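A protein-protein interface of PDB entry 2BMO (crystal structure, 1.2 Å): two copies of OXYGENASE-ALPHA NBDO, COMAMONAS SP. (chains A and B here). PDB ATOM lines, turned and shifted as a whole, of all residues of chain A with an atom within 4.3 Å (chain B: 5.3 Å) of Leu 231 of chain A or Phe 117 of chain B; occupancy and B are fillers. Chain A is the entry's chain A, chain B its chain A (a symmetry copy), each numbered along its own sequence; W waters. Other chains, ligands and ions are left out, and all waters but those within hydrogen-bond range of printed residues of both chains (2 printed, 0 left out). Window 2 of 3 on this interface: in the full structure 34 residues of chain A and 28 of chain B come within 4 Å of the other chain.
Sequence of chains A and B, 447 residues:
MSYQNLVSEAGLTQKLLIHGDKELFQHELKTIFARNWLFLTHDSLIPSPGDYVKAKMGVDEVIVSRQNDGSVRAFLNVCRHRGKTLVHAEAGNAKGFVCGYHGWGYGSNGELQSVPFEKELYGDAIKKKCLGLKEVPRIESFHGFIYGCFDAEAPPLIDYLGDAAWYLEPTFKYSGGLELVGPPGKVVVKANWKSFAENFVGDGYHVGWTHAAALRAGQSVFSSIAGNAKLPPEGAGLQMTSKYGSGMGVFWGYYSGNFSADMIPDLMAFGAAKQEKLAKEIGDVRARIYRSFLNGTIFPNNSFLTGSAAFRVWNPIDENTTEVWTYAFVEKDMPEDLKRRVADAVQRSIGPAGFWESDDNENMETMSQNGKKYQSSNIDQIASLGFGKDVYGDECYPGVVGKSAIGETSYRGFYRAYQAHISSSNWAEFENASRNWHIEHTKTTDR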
ATOM      1  N   TYR A 205      30.317 -22.565 -12.725  1.00  0.00           N
ATOM      2  CA  TYR A 205      29.858 -21.309 -12.130  1.00  0.00           C
ATOM      3  C   TYR A 205      30.890 -20.179 -12.212  1.00  0.00           C
ATOM      4  O   TYR A 205      30.520 -19.015 -12.380  1.00  0.00           O
ATOM      5  CB  TYR A 205      29.497 -21.590 -10.673  1.00  0.00           C
ATOM      6  CG  TYR A 205      28.670 -20.568  -9.899  1.00  0.00           C
ATOM      7  CD1 TYR A 205      27.905 -19.576 -10.524  1.00  0.00           C
ATOM      8  CD2 TYR A 205      28.618 -20.655  -8.515  1.00  0.00           C
ATOM      9  CE1 TYR A 205      27.138 -18.672  -9.757  1.00  0.00           C
ATOM     10  CE2 TYR A 205      27.856 -19.784  -7.753  1.00  0.00           C
ATOM     11  CZ  TYR A 205      27.126 -18.803  -8.369  1.00  0.00           C
ATOM     12  OH  TYR A 205      26.381 -17.962  -7.571  1.00  0.00           O
ATOM     13  N   ILE A 225      27.965 -16.910 -21.187  1.00  0.00           N
ATOM     14  CA  ILE A 225      27.712 -16.872 -19.742  1.00  0.00           C
ATOM     15  C   ILE A 225      28.489 -15.770 -19.020  1.00  0.00           C
ATOM     16  O   ILE A 225      28.556 -15.752 -17.793  1.00  0.00           O
ATOM     17  CB  ILE A 225      27.909 -18.260 -19.070  1.00  0.00           C
ATOM     18  CG1 ILE A 225      29.359 -18.755 -19.191  1.00  0.00           C
ATOM     19  CG2 ILE A 225      26.905 -19.253 -19.650  1.00  0.00           C
ATOM     20  CD1 ILE A 225      29.585 -20.128 -18.578  1.00  0.00           C
ATOM     21  N   ASN A 228      27.980 -14.079 -15.451  1.00  0.00           N
ATOM     22  CA  ASN A 228      26.963 -14.958 -14.855  1.00  0.00           C
ATOM     23  C   ASN A 228      25.557 -14.372 -14.978  1.00  0.00           C
ATOM     24  O   ASN A 228      24.734 -14.502 -14.073  1.00  0.00           O
ATOM     25  CB  ASN A 228      27.314 -15.309 -13.404  1.00  0.00           C
ATOM     26  CG  ASN A 228      28.426 -16.337 -13.318  1.00  0.00           C
ATOM     27  OD1 ASN A 228      28.719 -17.016 -14.301  1.00  0.00           O
ATOM     28  ND2 ASN A 228      29.053 -16.457 -12.153  1.00  0.00           N
ATOM     29  N   ALA A 229      25.304 -13.734 -16.117  1.00  0.00           N
ATOM     30  CA  ALA A 229      24.059 -13.002 -16.340  1.00  0.00           C
ATOM     31  C   ALA A 229      22.981 -13.913 -16.915  1.00  0.00           C
ATOM     32  O   ALA A 229      21.805 -13.817 -16.527  1.00  0.00           O
ATOM     33  CB  ALA A 229      24.306 -11.812 -17.262  1.00  0.00           C
ATOM     34  N   LYS A 230      23.387 -14.795 -17.833  1.00  0.00           N
ATOM     35  CA  LYS A 230      22.469 -15.696 -18.530  1.00  0.00           C
ATOM     36  C   LYS A 230      23.064 -17.088 -18.686  1.00  0.00           C
ATOM     37  O   LYS A 230      24.282 -17.246 -18.829  1.00  0.00           O
ATOM     38  CB  LYS A 230      22.125 -15.147 -19.922  1.00  0.00           C
ATOM     39  CG  LYS A 230      21.345 -13.839 -19.927  1.00  0.00           C
ATOM     40  N   LEU A 231      22.196 -18.095 -18.676  1.00  0.00           N
ATOM     41  CA  LEU A 231      22.605 -19.467 -18.942  1.00  0.00           C
ATOM     42  C   LEU A 231      22.892 -19.617 -20.437  1.00  0.00           C
ATOM     43  O   LEU A 231      22.457 -18.783 -21.240  1.00  0.00           O
ATOM     44  CB  LEU A 231      21.510 -20.439 -18.478  1.00  0.00           C
ATOM     45  CG  LEU A 231      21.246 -20.500 -16.967  1.00  0.00           C
ATOM     46  CD1 LEU A 231      19.995 -21.312 -16.669  1.00  0.00           C
ATOM     47  CD2 LEU A 231      22.448 -21.053 -16.201  1.00  0.00           C
ATOM     48  N   PRO A 232      23.643 -20.665 -20.827  1.00  0.00           N
ATOM     49  CA  PRO A 232      23.917 -20.846 -22.255  1.00  0.00           C
ATOM     50  C   PRO A 232      22.613 -21.032 -23.042  1.00  0.00           C
ATOM     51  O   PRO A 232      21.676 -21.647 -22.523  1.00  0.00           O
ATOM     52  CB  PRO A 232      24.742 -22.139 -22.300  1.00  0.00           C
ATOM     53  CG  PRO A 232      25.277 -22.314 -20.924  1.00  0.00           C
ATOM     54  CD  PRO A 232      24.260 -21.723 -20.005  1.00  0.00           C
ATOM     55  N   PRO A 233      22.538 -20.498 -24.275  1.00  0.00           N
ATOM     56  CA  PRO A 233      21.329 -20.707 -25.090  1.00  0.00           C
ATOM     57  C   PRO A 233      21.055 -22.180 -25.400  1.00  0.00           C
ATOM     58  O   PRO A 233      19.908 -22.551 -25.660  1.00  0.00           O
ATOM     59  CB  PRO A 233      21.620 -19.936 -26.384  1.00  0.00           C
ATOM     60  CG  PRO A 233      23.075 -19.669 -26.383  1.00  0.00           C
ATOM     61  CD  PRO A 233      23.527 -19.643 -24.956  1.00  0.00           C
ATOM     62  N   ILE A 406      26.668 -25.628 -14.478  1.00  0.00           N
ATOM     63  CA  ILE A 406      26.848 -24.647 -13.419  1.00  0.00           C
ATOM     64  C   ILE A 406      26.125 -25.274 -12.236  1.00  0.00           C
ATOM     65  O   ILE A 406      24.905 -25.163 -12.097  1.00  0.00           O
ATOM     66  CB  ILE A 406      26.259 -23.281 -13.814  1.00  0.00           C
ATOM     67  CG1 ILE A 406      26.976 -22.755 -15.060  1.00  0.00           C
ATOM     68  CG2 ILE A 406      26.357 -22.295 -12.655  1.00  0.00           C
ATOM     69  CD1 ILE A 406      26.295 -21.587 -15.739  1.00  0.00           C
ATOM     70  N   VAL B 115      23.675 -12.963  -5.304  1.00  0.00           N
ATOM     71  CA  VAL B 115      24.217 -14.257  -5.679  1.00  0.00           C
ATOM     72  C   VAL B 115      23.873 -14.459  -7.146  1.00  0.00           C
ATOM     73  O   VAL B 115      22.694 -14.583  -7.483  1.00  0.00           O
ATOM     74  CB  VAL B 115      23.602 -15.378  -4.808  1.00  0.00           C
ATOM     75  CG1 VAL B 115      23.927 -16.757  -5.355  1.00  0.00           C
ATOM     76  CG2 VAL B 115      24.074 -15.260  -3.370  1.00  0.00           C
ATOM     77  N   PRO B 116      24.879 -14.446  -8.042  1.00  0.00           N
ATOM     78  CA  PRO B 116      24.590 -14.691  -9.455  1.00  0.00           C
ATOM     79  C   PRO B 116      23.909 -16.043  -9.659  1.00  0.00           C
ATOM     80  O   PRO B 116      24.249 -17.025  -8.993  1.00  0.00           O
ATOM     81  CB  PRO B 116      25.977 -14.655 -10.107  1.00  0.00           C
ATOM     82  CG  PRO B 116      26.787 -13.786  -9.176  1.00  0.00           C
ATOM     83  CD  PRO B 116      26.315 -14.170  -7.818  1.00  0.00           C
ATOM     84  N   PHE B 117      22.929 -16.063 -10.560  1.00  0.00           N
ATOM     85  CA  PHE B 117      22.088 -17.245 -10.826  1.00  0.00           C
ATOM     86  C   PHE B 117      21.248 -17.715  -9.630  1.00  0.00           C
ATOM     87  O   PHE B 117      20.854 -18.886  -9.567  1.00  0.00           O
ATOM     88  CB  PHE B 117      22.913 -18.419 -11.400  1.00  0.00           C
ATOM     89  CG  PHE B 117      23.477 -18.162 -12.769  1.00  0.00           C
ATOM     90  CD1 PHE B 117      24.824 -18.403 -13.036  1.00  0.00           C
ATOM     91  CD2 PHE B 117      22.663 -17.694 -13.801  1.00  0.00           C
ATOM     92  CE1 PHE B 117      25.347 -18.185 -14.307  1.00  0.00           C
ATOM     93  CE2 PHE B 117      23.179 -17.463 -15.072  1.00  0.00           C
ATOM     94  CZ  PHE B 117      24.523 -17.715 -15.329  1.00  0.00           C
ATOM     95  N   GLU B 118      20.961 -16.813  -8.690  1.00  0.00           N
ATOM     96  CA  GLU B 118      20.137 -17.183  -7.538  1.00  0.00           C
ATOM     97  C   GLU B 118      18.766 -17.715  -7.971  1.00  0.00           C
ATOM     98  O   GLU B 118      18.368 -18.803  -7.559  1.00  0.00           O
ATOM     99  CB  GLU B 118      19.964 -16.028  -6.544  1.00  0.00           C
ATOM    100  CG  GLU B 118      19.214 -16.463  -5.279  1.00  0.00           C
ATOM    101  CD  GLU B 118      18.996 -15.352  -4.270  1.00  0.00           C
ATOM    102  OE1 GLU B 118      18.304 -15.614  -3.262  1.00  0.00           O
ATOM    103  OE2 GLU B 118      19.504 -14.234  -4.475  1.00  0.00           O
ATOM    104  N   LYS B 119      18.070 -16.951  -8.809  1.00  0.00           N
ATOM    105  CA  LYS B 119      16.733 -17.328  -9.276  1.00  0.00           C
ATOM    106  C   LYS B 119      16.767 -18.565 -10.177  1.00  0.00           C
ATOM    107  O   LYS B 119      15.944 -19.475 -10.024  1.00  0.00           O
ATOM    108  CB  LYS B 119      16.073 -16.150 -10.002  1.00  0.00           C
ATOM    109  CG  LYS B 119      14.647 -16.421 -10.494  1.00  0.00           C
ATOM    110  N   GLU B 120      17.720 -18.598 -11.103  1.00  0.00           N
ATOM    111  CA  GLU B 120      17.777 -19.650 -12.115  1.00  0.00           C
ATOM    112  C   GLU B 120      18.233 -20.995 -11.555  1.00  0.00           C
ATOM    113  O   GLU B 120      17.736 -22.042 -11.980  1.00  0.00           O
ATOM    114  CB  GLU B 120      18.681 -19.231 -13.283  1.00  0.00           C
ATOM    115  CG  GLU B 120      18.177 -18.037 -14.090  1.00  0.00           C
ATOM    116  CD  GLU B 120      18.606 -16.687 -13.520  1.00  0.00           C
ATOM    117  OE1 GLU B 120      19.182 -16.647 -12.412  1.00  0.00           O
ATOM    118  OE2 GLU B 120      18.356 -15.656 -14.186  1.00  0.00           O
ATOM    119  N   LEU B 121      19.166 -20.977 -10.602  1.00  0.00           N
ATOM    120  CA  LEU B 121      19.826 -22.215 -10.182  1.00  0.00           C
ATOM    121  C   LEU B 121      19.745 -22.562  -8.700  1.00  0.00           C
ATOM    122  O   LEU B 121      19.718 -23.740  -8.346  1.00  0.00           O
ATOM    123  CB  LEU B 121      21.287 -22.237 -10.651  1.00  0.00           C
ATOM    124  CG  LEU B 121      21.543 -22.201 -12.161  1.00  0.00           C
ATOM    125  CD1 LEU B 121      23.029 -22.106 -12.426  1.00  0.00           C
ATOM    126  CD2 LEU B 121      20.943 -23.417 -12.882  1.00  0.00           C
ATOM    127  N   TYR B 122      19.716 -21.556  -7.833  1.00  0.00           N
ATOM    128  CA  TYR B 122      19.643 -21.821  -6.399  1.00  0.00           C
ATOM    129  C   TYR B 122      18.215 -22.005  -5.897  1.00  0.00           C
ATOM    130  O   TYR B 122      17.913 -23.013  -5.264  1.00  0.00           O
ATOM    131  CB  TYR B 122      20.340 -20.727  -5.588  1.00  0.00           C
ATOM    132  CG  TYR B 122      21.838 -20.895  -5.428  1.00  0.00           C
ATOM    133  CD1 TYR B 122      22.717 -20.092  -6.146  1.00  0.00           C
ATOM    134  CD2 TYR B 122      22.373 -21.834  -4.543  1.00  0.00           C
ATOM    135  CE1 TYR B 122      24.089 -20.217  -5.998  1.00  0.00           C
ATOM    136  CE2 TYR B 122      23.759 -21.976  -4.391  1.00  0.00           C
ATOM    137  CZ  TYR B 122      24.606 -21.154  -5.127  1.00  0.00           C
ATOM    138  OH  TYR B 122      25.977 -21.251  -5.004  1.00  0.00           O
HETATM  139  O   HOH W   1      19.412 -15.100 -16.564  1.00  0.00           O
HETATM  140  O   HOH W   2      22.918 -13.705 -12.347  1.00  0.00           O
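The backbone carbonyl oxygen of Pro 116 of chain B is in hydrogen-bond range of the side-chain hydroxyl of Tyr 205 of chain A (2.7 Å).
The backbone carbonyl oxygen of Tyr 205 of chain A sits at hydrogen-bond distance from the side-chain amide nitrogen of Asn 228 of chain A (3.0 Å).
The backbone NH (N) of Tyr 122 of chain B lies within hydrogen-bond range of the backbone carbonyl oxygen (O) of Phe 117 of chain B.
Among the printed residues, merely in contact across the chains: Tyr 205 of chain A with Val 115 of chain B, Tyr 205 of chain A with Tyr 122 of chain B, Asn 228 of chain A with Pro 116 of chain B, Asn 228 of chain A with Phe 117 of chain B, Lys 230 of chain A with Phe 117 of chain B, Leu 231 of chain A with Phe 117 of chain B, Leu 231 of chain A with Leu 121 of chain B, Ile 406 of chain A with Phe 117 of chain B and Ile 406 of chain A with Leu 121 of chain B.
Of the printed residues of chain B, Tyr 205 of chain A touches Val 115 (3.5 Å), Pro 116 (2.7 Å) and Tyr 122 (3.6 Å).
Printed residues of chain B within 4 Å of Asn 228 of chain A: Pro 116 (3.6 Å) and Phe 117 (3.5 Å).
Printed residues of chain B within 4 Å of Lys 230 of chain A: Phe 117 (3.5 Å).
Leu 231 of chain A touches just these residues of chain B: Phe 117 (3.8 Å) and Leu 121 (3.96 Å).
Of the printed residues of chain A, Pro 116 of chain B touches Tyr 205 (2.7 Å) and Asn 228 (3.6 Å).
Printed residues of chain A within 4 Å of Phe 117 of chain B: Asn 228 (3.5 Å), Lys 230 (3.5 Å), Leu 231 (3.8 Å) and Ile 406 (3.8 Å).
Lys 119 of chain B touches none of the printed residues of chain A.
Glu 120 of chain B touches none of the printed residues of chain A.
The nearest residue of chain B that does not touch Leu 231 of chain A is Glu 120 of chain B (4.2 Å).
The nearest printed residue of chain A that does not touch Phe 117 of chain B is Ala 229 of chain A (4.005 Å).
The nearest printed residue of chain B that does not touch Lys 230 of chain A is Glu 120 of chain B (6.0 Å).
Of the 9 printed residues of chain A, 5 touch a printed residue of chain B.
Printed residues of chain A that touch a printed residue of chain B: Tyr 205, Asn 228, Lys 230, Leu 231 and Ile 406.
Hydrophobic or aromatic side chains of chain A within 4 Å of the printed part of chain B: Tyr 205, Leu 231 and Ile 406.
Among the printed residues, 10 pairs touch across the chains.
Among the printed residues, no Asp or Glu carboxylate lies within 4 Å of a Lys or Arg side-chain nitrogen of the other chain.
No position is printed for both chains.
Of the 10 pairs that touch across the chains among the printed residues, none has its exchanged pair printed and touching as well.
Water W2 lies within hydrogen-bond range of O of Asn 228 of chain A (2.6 Å) and N of Phe 117 of chain B (3.0 Å).
Water W1 lies within hydrogen-bond range of OE2 of Glu 120 of chain B and O of Ala 229 of chain A.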
